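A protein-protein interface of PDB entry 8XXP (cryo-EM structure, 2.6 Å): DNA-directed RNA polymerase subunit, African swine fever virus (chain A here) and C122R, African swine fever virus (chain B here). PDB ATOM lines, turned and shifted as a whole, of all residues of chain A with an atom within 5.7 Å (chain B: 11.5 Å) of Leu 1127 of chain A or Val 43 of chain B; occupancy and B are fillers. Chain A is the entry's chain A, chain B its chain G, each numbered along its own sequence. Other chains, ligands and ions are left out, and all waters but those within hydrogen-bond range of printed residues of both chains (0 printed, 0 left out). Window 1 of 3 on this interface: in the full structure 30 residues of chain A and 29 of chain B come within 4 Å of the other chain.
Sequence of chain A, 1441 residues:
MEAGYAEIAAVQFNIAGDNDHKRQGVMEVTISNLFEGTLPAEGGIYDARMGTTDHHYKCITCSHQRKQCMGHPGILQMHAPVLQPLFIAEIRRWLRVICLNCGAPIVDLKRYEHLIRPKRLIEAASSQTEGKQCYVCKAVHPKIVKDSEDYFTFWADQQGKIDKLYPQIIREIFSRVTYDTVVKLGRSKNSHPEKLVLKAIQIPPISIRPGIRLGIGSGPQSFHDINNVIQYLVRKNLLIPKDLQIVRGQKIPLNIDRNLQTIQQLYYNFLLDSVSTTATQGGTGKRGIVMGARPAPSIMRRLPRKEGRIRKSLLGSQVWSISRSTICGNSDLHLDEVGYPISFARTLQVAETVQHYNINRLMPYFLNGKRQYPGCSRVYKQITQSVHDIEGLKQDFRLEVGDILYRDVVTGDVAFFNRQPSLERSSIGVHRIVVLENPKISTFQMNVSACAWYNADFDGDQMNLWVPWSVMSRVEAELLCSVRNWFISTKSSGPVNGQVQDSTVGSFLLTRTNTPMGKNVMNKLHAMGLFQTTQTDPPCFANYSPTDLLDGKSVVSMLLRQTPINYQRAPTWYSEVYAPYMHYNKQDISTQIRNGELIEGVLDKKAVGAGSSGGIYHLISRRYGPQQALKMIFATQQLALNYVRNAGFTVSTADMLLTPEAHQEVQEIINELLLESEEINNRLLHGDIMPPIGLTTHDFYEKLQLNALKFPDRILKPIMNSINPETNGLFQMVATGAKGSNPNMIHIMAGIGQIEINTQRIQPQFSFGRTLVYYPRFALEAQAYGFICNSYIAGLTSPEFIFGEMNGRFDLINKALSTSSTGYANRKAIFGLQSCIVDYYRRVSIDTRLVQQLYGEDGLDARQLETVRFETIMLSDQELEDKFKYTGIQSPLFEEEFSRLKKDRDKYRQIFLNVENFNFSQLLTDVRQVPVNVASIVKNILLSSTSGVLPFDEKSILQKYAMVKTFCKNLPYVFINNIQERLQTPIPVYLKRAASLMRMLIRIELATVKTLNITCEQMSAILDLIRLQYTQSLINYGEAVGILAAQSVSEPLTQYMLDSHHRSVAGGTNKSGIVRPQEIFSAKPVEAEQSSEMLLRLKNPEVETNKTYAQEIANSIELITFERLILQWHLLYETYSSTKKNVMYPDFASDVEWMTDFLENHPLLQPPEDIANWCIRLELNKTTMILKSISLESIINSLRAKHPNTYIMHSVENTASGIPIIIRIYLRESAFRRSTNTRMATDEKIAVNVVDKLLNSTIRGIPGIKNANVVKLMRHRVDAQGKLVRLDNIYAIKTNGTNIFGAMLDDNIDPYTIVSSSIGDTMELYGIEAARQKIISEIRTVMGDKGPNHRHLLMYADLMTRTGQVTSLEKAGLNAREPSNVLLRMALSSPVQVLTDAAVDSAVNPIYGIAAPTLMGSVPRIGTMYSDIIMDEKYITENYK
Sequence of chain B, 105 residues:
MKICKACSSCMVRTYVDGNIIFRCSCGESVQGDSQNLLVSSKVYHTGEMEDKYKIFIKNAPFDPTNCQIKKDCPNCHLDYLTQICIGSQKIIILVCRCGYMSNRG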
ATOM      1  N   LEU A1125      -3.343   0.693 -21.951  1.00  0.00           N
ATOM      2  CA  LEU A1125      -3.288  -0.360 -20.950  1.00  0.00           C
ATOM      3  C   LEU A1125      -3.904   0.048 -19.622  1.00  0.00           C
ATOM      4  O   LEU A1125      -3.833  -0.720 -18.660  1.00  0.00           O
ATOM      5  CB  LEU A1125      -1.835  -0.782 -20.728  1.00  0.00           C
ATOM      6  CG  LEU A1125      -1.031  -1.013 -22.003  1.00  0.00           C
ATOM      7  CD1 LEU A1125       0.446  -1.087 -21.696  1.00  0.00           C
ATOM      8  CD2 LEU A1125      -1.498  -2.279 -22.677  1.00  0.00           C
ATOM      9  N   ILE A1126      -4.515   1.225 -19.550  1.00  0.00           N
ATOM     10  CA  ILE A1126      -4.932   1.832 -18.294  1.00  0.00           C
ATOM     11  C   ILE A1126      -6.449   1.826 -18.219  1.00  0.00           C
ATOM     12  O   ILE A1126      -7.126   2.248 -19.162  1.00  0.00           O
ATOM     13  CB  ILE A1126      -4.383   3.260 -18.173  1.00  0.00           C
ATOM     14  CG1 ILE A1126      -2.878   3.215 -17.963  1.00  0.00           C
ATOM     15  CG2 ILE A1126      -5.054   4.003 -17.043  1.00  0.00           C
ATOM     16  CD1 ILE A1126      -2.228   4.533 -18.133  1.00  0.00           C
ATOM     17  N   LEU A1127      -6.981   1.339 -17.098  1.00  0.00           N
ATOM     18  CA  LEU A1127      -8.412   1.454 -16.849  1.00  0.00           C
ATOM     19  C   LEU A1127      -8.778   2.848 -16.364  1.00  0.00           C
ATOM     20  O   LEU A1127      -9.730   3.453 -16.866  1.00  0.00           O
ATOM     21  CB  LEU A1127      -8.855   0.409 -15.829  1.00  0.00           C
ATOM     22  CG  LEU A1127      -8.909  -1.030 -16.331  1.00  0.00           C
ATOM     23  CD1 LEU A1127      -8.949  -1.987 -15.166  1.00  0.00           C
ATOM     24  CD2 LEU A1127     -10.114  -1.224 -17.227  1.00  0.00           C
ATOM     25  N   GLN A1128      -8.036   3.371 -15.396  1.00  0.00           N
ATOM     26  CA  GLN A1128      -8.331   4.679 -14.835  1.00  0.00           C
ATOM     27  C   GLN A1128      -7.065   5.241 -14.218  1.00  0.00           C
ATOM     28  O   GLN A1128      -6.176   4.493 -13.810  1.00  0.00           O
ATOM     29  CB  GLN A1128      -9.439   4.595 -13.787  1.00  0.00           C
ATOM     30  CG  GLN A1128      -9.096   3.714 -12.607  1.00  0.00           C
ATOM     31  CD  GLN A1128     -10.124   3.803 -11.507  1.00  0.00           C
ATOM     32  OE1 GLN A1128     -11.189   4.391 -11.687  1.00  0.00           O
ATOM     33  NE2 GLN A1128      -9.811   3.228 -10.353  1.00  0.00           N
ATOM     34  N   TRP A1129      -6.989   6.566 -14.159  1.00  0.00           N
ATOM     35  CA  TRP A1129      -5.867   7.233 -13.524  1.00  0.00           C
ATOM     36  C   TRP A1129      -6.372   8.408 -12.704  1.00  0.00           C
ATOM     37  O   TRP A1129      -7.408   8.998 -13.010  1.00  0.00           O
ATOM     38  CB  TRP A1129      -4.822   7.698 -14.542  1.00  0.00           C
ATOM     39  CG  TRP A1129      -5.280   8.730 -15.511  1.00  0.00           C
ATOM     40  CD1 TRP A1129      -5.695   8.518 -16.785  1.00  0.00           C
ATOM     41  CD2 TRP A1129      -5.348  10.143 -15.297  1.00  0.00           C
ATOM     42  NE1 TRP A1129      -6.028   9.705 -17.380  1.00  0.00           N
ATOM     43  CE2 TRP A1129      -5.825  10.720 -16.485  1.00  0.00           C
ATOM     44  CE3 TRP A1129      -5.061  10.975 -14.212  1.00  0.00           C
ATOM     45  CZ2 TRP A1129      -6.016  12.089 -16.623  1.00  0.00           C
ATOM     46  CZ3 TRP A1129      -5.252  12.331 -14.351  1.00  0.00           C
ATOM     47  CH2 TRP A1129      -5.724  12.876 -15.546  1.00  0.00           C
ATOM     48  N   HIS A1130      -5.623   8.738 -11.655  1.00  0.00           N
ATOM     49  CA  HIS A1130      -5.991   9.801 -10.730  1.00  0.00           C
ATOM     50  C   HIS A1130      -4.740  10.570 -10.351  1.00  0.00           C
ATOM     51  O   HIS A1130      -3.866  10.031  -9.669  1.00  0.00           O
ATOM     52  CB  HIS A1130      -6.664   9.236  -9.477  1.00  0.00           C
ATOM     53  CG  HIS A1130      -7.719   8.220  -9.766  1.00  0.00           C
ATOM     54  ND1 HIS A1130      -8.997   8.562 -10.148  1.00  0.00           N
ATOM     55  CD2 HIS A1130      -7.685   6.867  -9.734  1.00  0.00           C
ATOM     56  CE1 HIS A1130      -9.706   7.464 -10.337  1.00  0.00           C
ATOM     57  NE2 HIS A1130      -8.933   6.422 -10.091  1.00  0.00           N
ATOM     58  N   GLU A1179      -4.577   2.439 -12.764  1.00  0.00           N
ATOM     59  CA  GLU A1179      -4.998   1.051 -12.668  1.00  0.00           C
ATOM     60  C   GLU A1179      -4.880   0.418 -14.046  1.00  0.00           C
ATOM     61  O   GLU A1179      -5.485   0.901 -15.007  1.00  0.00           O
ATOM     62  CB  GLU A1179      -6.431   0.949 -12.148  1.00  0.00           C
ATOM     63  CG  GLU A1179      -6.991  -0.462 -12.101  1.00  0.00           C
ATOM     64  CD  GLU A1179      -8.324  -0.529 -11.377  1.00  0.00           C
ATOM     65  OE1 GLU A1179      -8.324  -0.582 -10.129  1.00  0.00           O
ATOM     66  OE2 GLU A1179      -9.373  -0.522 -12.054  1.00  0.00           O
ATOM     67  N   LEU A1180      -4.102  -0.652 -14.139  1.00  0.00           N
ATOM     68  CA  LEU A1180      -3.835  -1.288 -15.418  1.00  0.00           C
ATOM     69  C   LEU A1180      -5.000  -2.167 -15.850  1.00  0.00           C
ATOM     70  O   LEU A1180      -5.761  -2.681 -15.027  1.00  0.00           O
ATOM     71  CB  LEU A1180      -2.562  -2.130 -15.354  1.00  0.00           C
ATOM     72  CG  LEU A1180      -1.206  -1.488 -15.648  1.00  0.00           C
ATOM     73  CD1 LEU A1180      -1.071  -1.145 -17.113  1.00  0.00           C
ATOM     74  CD2 LEU A1180      -1.021  -0.261 -14.820  1.00  0.00           C
ATOM     75  N   ASN A1181      -5.126  -2.335 -17.162  1.00  0.00           N
ATOM     76  CA  ASN A1181      -6.112  -3.229 -17.758  1.00  0.00           C
ATOM     77  C   ASN A1181      -5.436  -4.572 -17.993  1.00  0.00           C
ATOM     78  O   ASN A1181      -4.686  -4.743 -18.955  1.00  0.00           O
ATOM     79  CB  ASN A1181      -6.657  -2.631 -19.050  1.00  0.00           C
ATOM     80  CG  ASN A1181      -7.805  -3.428 -19.627  1.00  0.00           C
ATOM     81  OD1 ASN A1181      -7.704  -4.638 -19.813  1.00  0.00           O
ATOM     82  ND2 ASN A1181      -8.904  -2.750 -19.925  1.00  0.00           N
ATOM     83  N   LYS A1182      -5.698  -5.534 -17.108  1.00  0.00           N
ATOM     84  CA  LYS A1182      -5.090  -6.850 -17.260  1.00  0.00           C
ATOM     85  C   LYS A1182      -5.624  -7.579 -18.485  1.00  0.00           C
ATOM     86  O   LYS A1182      -4.908  -8.389 -19.081  1.00  0.00           O
ATOM     87  CB  LYS A1182      -5.316  -7.683 -16.003  1.00  0.00           C
ATOM     88  CG  LYS A1182      -4.372  -7.327 -14.866  1.00  0.00           C
ATOM     89  CD  LYS A1182      -4.148  -8.497 -13.920  1.00  0.00           C
ATOM     90  CE  LYS A1182      -2.944  -9.339 -14.330  1.00  0.00           C
ATOM     91  NZ  LYS A1182      -3.035  -9.877 -15.713  1.00  0.00           N
ATOM     92  N   LEU B  38      -7.620  14.972  -4.710  1.00  0.00           N
ATOM     93  CA  LEU B  38      -7.858  14.444  -6.052  1.00  0.00           C
ATOM     94  C   LEU B  38      -7.821  15.608  -7.034  1.00  0.00           C
ATOM     95  O   LEU B  38      -8.827  16.284  -7.252  1.00  0.00           O
ATOM     96  CB  LEU B  38      -9.191  13.708  -6.104  1.00  0.00           C
ATOM     97  CG  LEU B  38      -9.478  12.716  -7.234  1.00  0.00           C
ATOM     98  CD1 LEU B  38      -9.868  13.420  -8.523  1.00  0.00           C
ATOM     99  CD2 LEU B  38      -8.288  11.818  -7.460  1.00  0.00           C
ATOM    100  N   SER B  40      -7.058  15.563 -10.419  1.00  0.00           N
ATOM    101  CA  SER B  40      -7.713  15.211 -11.669  1.00  0.00           C
ATOM    102  C   SER B  40      -7.893  13.704 -11.711  1.00  0.00           C
ATOM    103  O   SER B  40      -7.340  12.971 -10.890  1.00  0.00           O
ATOM    104  CB  SER B  40      -6.922  15.699 -12.886  1.00  0.00           C
ATOM    105  OG  SER B  40      -7.149  17.077 -13.115  1.00  0.00           O
ATOM    106  N   SER B  41      -8.691  13.246 -12.667  1.00  0.00           N
ATOM    107  CA  SER B  41      -8.977  11.826 -12.784  1.00  0.00           C
ATOM    108  C   SER B  41      -9.489  11.546 -14.186  1.00  0.00           C
ATOM    109  O   SER B  41      -9.740  12.462 -14.972  1.00  0.00           O
ATOM    110  CB  SER B  41      -9.988  11.373 -11.729  1.00  0.00           C
ATOM    111  OG  SER B  41     -10.322  10.011 -11.897  1.00  0.00           O
ATOM    112  N   LYS B  42      -9.620  10.257 -14.494  1.00  0.00           N
ATOM    113  CA  LYS B  42     -10.282   9.817 -15.714  1.00  0.00           C
ATOM    114  C   LYS B  42     -10.546   8.327 -15.608  1.00  0.00           C
ATOM    115  O   LYS B  42      -9.638   7.560 -15.284  1.00  0.00           O
ATOM    116  CB  LYS B  42      -9.439  10.116 -16.955  1.00  0.00           C
ATOM    117  CG  LYS B  42     -10.123   9.752 -18.257  1.00  0.00           C
ATOM    118  CD  LYS B  42      -9.519  10.522 -19.415  1.00  0.00           C
ATOM    119  CE  LYS B  42     -10.526  10.736 -20.531  1.00  0.00           C
ATOM    120  NZ  LYS B  42     -10.730   9.514 -21.350  1.00  0.00           N
ATOM    121  N   VAL B  43     -11.785   7.925 -15.874  1.00  0.00           N
ATOM    122  CA  VAL B  43     -12.171   6.524 -15.956  1.00  0.00           C
ATOM    123  C   VAL B  43     -12.496   6.228 -17.411  1.00  0.00           C
ATOM    124  O   VAL B  43     -13.227   6.989 -18.054  1.00  0.00           O
ATOM    125  CB  VAL B  43     -13.365   6.208 -15.042  1.00  0.00           C
ATOM    126  CG1 VAL B  43     -13.651   4.718 -15.047  1.00  0.00           C
ATOM    127  CG2 VAL B  43     -13.094   6.700 -13.632  1.00  0.00           C
ATOM    128  N   TYR B  44     -11.947   5.137 -17.931  1.00  0.00           N
ATOM    129  CA  TYR B  44     -11.965   4.874 -19.364  1.00  0.00           C
ATOM    130  C   TYR B  44     -13.147   3.975 -19.715  1.00  0.00           C
ATOM    131  O   TYR B  44     -13.167   2.795 -19.354  1.00  0.00           O
ATOM    132  CB  TYR B  44     -10.641   4.255 -19.797  1.00  0.00           C
ATOM    133  CG  TYR B  44      -9.576   5.292 -20.048  1.00  0.00           C
ATOM    134  CD1 TYR B  44      -9.616   6.088 -21.178  1.00  0.00           C
ATOM    135  CD2 TYR B  44      -8.552   5.498 -19.139  1.00  0.00           C
ATOM    136  CE1 TYR B  44      -8.657   7.044 -21.409  1.00  0.00           C
ATOM    137  CE2 TYR B  44      -7.589   6.454 -19.361  1.00  0.00           C
ATOM    138  CZ  TYR B  44      -7.646   7.224 -20.498  1.00  0.00           C
ATOM    139  OH  TYR B  44      -6.690   8.182 -20.733  1.00  0.00           O
ATOM    140  N   HIS B  45     -14.130   4.550 -20.415  1.00  0.00           N
ATOM    141  CA  HIS B  45     -15.263   3.826 -21.006  1.00  0.00           C
ATOM    142  C   HIS B  45     -15.928   2.871 -20.014  1.00  0.00           C
ATOM    143  O   HIS B  45     -16.305   1.750 -20.360  1.00  0.00           O
ATOM    144  CB  HIS B  45     -14.843   3.101 -22.294  1.00  0.00           C
ATOM    145  CG  HIS B  45     -13.900   1.955 -22.085  1.00  0.00           C
ATOM    146  ND1 HIS B  45     -12.531   2.112 -22.069  1.00  0.00           N
ATOM    147  CD2 HIS B  45     -14.125   0.629 -21.925  1.00  0.00           C
ATOM    148  CE1 HIS B  45     -11.956   0.938 -21.882  1.00  0.00           C
ATOM    149  NE2 HIS B  45     -12.900   0.021 -21.792  1.00  0.00           N
ATOM    150  N   THR B  46     -16.108   3.323 -18.776  1.00  0.00           N
ATOM    151  CA  THR B  46     -16.684   2.497 -17.725  1.00  0.00           C
ATOM    152  C   THR B  46     -17.778   3.261 -16.992  1.00  0.00           C
ATOM    153  O   THR B  46     -17.605   4.435 -16.651  1.00  0.00           O
ATOM    154  CB  THR B  46     -15.606   2.045 -16.733  1.00  0.00           C
ATOM    155  OG1 THR B  46     -14.499   1.488 -17.454  1.00  0.00           O
ATOM    156  CG2 THR B  46     -16.159   1.000 -15.777  1.00  0.00           C
ATOM    157  N   GLY B  47     -18.904   2.587 -16.757  1.00  0.00           N
ATOM    158  CA  GLY B  47     -19.970   3.127 -15.933  1.00  0.00           C
ATOM    159  C   GLY B  47     -20.862   4.154 -16.599  1.00  0.00           C
ATOM    160  O   GLY B  47     -20.901   5.313 -16.175  1.00  0.00           O
ATOM    161  N   GLU B  48     -21.587   3.750 -17.635  1.00  0.00           N
ATOM    162  CA  GLU B  48     -22.480   4.661 -18.344  1.00  0.00           C
ATOM    163  C   GLU B  48     -23.641   3.857 -18.922  1.00  0.00           C
ATOM    164  O   GLU B  48     -23.930   2.745 -18.466  1.00  0.00           O
ATOM    165  CB  GLU B  48     -21.717   5.444 -19.424  1.00  0.00           C
ATOM    166  CG  GLU B  48     -22.179   6.885 -19.566  1.00  0.00           C
ATOM    167  CD  GLU B  48     -21.860   7.465 -20.924  1.00  0.00           C
ATOM    168  OE1 GLU B  48     -20.877   7.016 -21.550  1.00  0.00           O
ATOM    169  OE2 GLU B  48     -22.598   8.369 -21.368  1.00  0.00           O
ATOM    170  N   ASP B  51     -27.379   4.748 -16.908  1.00  0.00           N
ATOM    171  CA  ASP B  51     -27.702   6.060 -16.357  1.00  0.00           C
ATOM    172  C   ASP B  51     -27.887   7.098 -17.453  1.00  0.00           C
ATOM    173  O   ASP B  51     -28.695   8.021 -17.304  1.00  0.00           O
ATOM    174  CB  ASP B  51     -26.608   6.506 -15.391  1.00  0.00           C
ATOM    175  CG  ASP B  51     -25.225   6.469 -16.018  1.00  0.00           C
ATOM    176  OD1 ASP B  51     -24.454   5.536 -15.707  1.00  0.00           O
ATOM    177  OD2 ASP B  51     -24.907   7.374 -16.820  1.00  0.00           O
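Leu 1127 of chain A touches two residues of chain B.
Ile 1126 of chain A touches one residue of chain B.
Gln 1128 of chain A touches two residues of chain B.
No residue of chain B comes within 4 Å of Glu 1179 of chain A.
No residue of chain B comes within 4 Å of Leu 1180 of chain A.
Of the printed residues of chain B, Trp 1129 of chain A touches Ser 40, Ser 41, Lys 42 and Tyr 44.
Of the printed residues of chain A, Tyr 44 of chain B touches Ile 1126, Leu 1127 and Trp 1129.
Of the printed residues of chain B, His 1130 of chain A touches Leu 38 (3.7 Å), Ser 40 (3.4 Å) and Ser 41 (2.6 Å).
Printed residues of chain A within 4 Å of Ser 41 of chain B: Trp 1129 (3.2 Å) and His 1130 (2.6 Å).
Of the printed residues of chain A, Lys 42 of chain B touches Gln 1128 (3.2 Å) and Trp 1129 (2.9 Å).
Asp 51 of chain B touches none of the printed residues of chain A.
Gly 47 of chain B touches none of the printed residues of chain A.
The nearest residue of chain B that does not touch Leu 1127 of chain A is Lys 42 of chain B (4.4 Å).
The nearest printed residue of chain A that does not touch Lys 42 of chain B is Leu 1127 of chain A (4.4 Å).
NE2 of His 1130 of chain A lies close to NE2 of Gln 1128 of chain A, 3.3 Å away.
O of Tyr 44 of chain B sits at hydrogen-bond distance from OG1 of Thr 46 of chain B, at 2.7 Å.
The backbone carbonyl oxygen (O) of Gln 1128 of chain A lies within hydrogen-bond range of the backbone NH (N) of Glu 1179 of chain A (2.8 Å).
N of Leu 1127 of chain A sits at hydrogen-bond distance from O of Glu 1179 of chain A, 2.6 Å away.
Ile 1126 of chain A touches Tyr 44 of chain B.
Leu 1127 of chain A touches Val 43 of chain B.
Lys 42 of chain B touches Gln 1128 of chain A.
Gln 1128 of chain A touches Val 43 of chain B (OE1 to CG2, 3.6 Å).
CZ3 of Trp 1129 of chain A touches C of Ser 40 of chain B (3.98 Å).
Tyr 44 of chain B touches Trp 1129 of chain A.
Leu 38 of chain B touches His 1130 of chain A (CD2 to CB, 3.7 Å).
O of Ser 40 of chain B touches CA of His 1130 of chain A, 3.4 Å away.
Printed residues of chain A that touch a printed residue of chain B: Ile 1126, Leu 1127, Gln 1128, Trp 1129 and His 1130.
Hydrophobic or aromatic side chains of chain B within 4 Å of the printed part of chain A: Leu 38, Val 43 and Tyr 44.
Among the printed residues, no Asp or Glu carboxylate lies within 4 Å of a Lys or Arg side-chain nitrogen of the other chain.
The backbone carbonyl oxygen (O) of Leu 1127 of chain A lies within hydrogen-bond range of the backbone NH (N) of Tyr 44 of chain B, at 3.0 Å.
A ring nitrogen (ND1) of His 1130 of chain A is in hydrogen-bond range of the side-chain hydroxyl (OG) of Ser 41 of chain B (2.6 Å).
N of Lys 42 of chain B lies within hydrogen-bond range of O of Trp 1129 of chain A (2.9 Å).
OG of Ser 41 of chain B lies close to O of Trp 1129 of chain A (3.3 Å).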
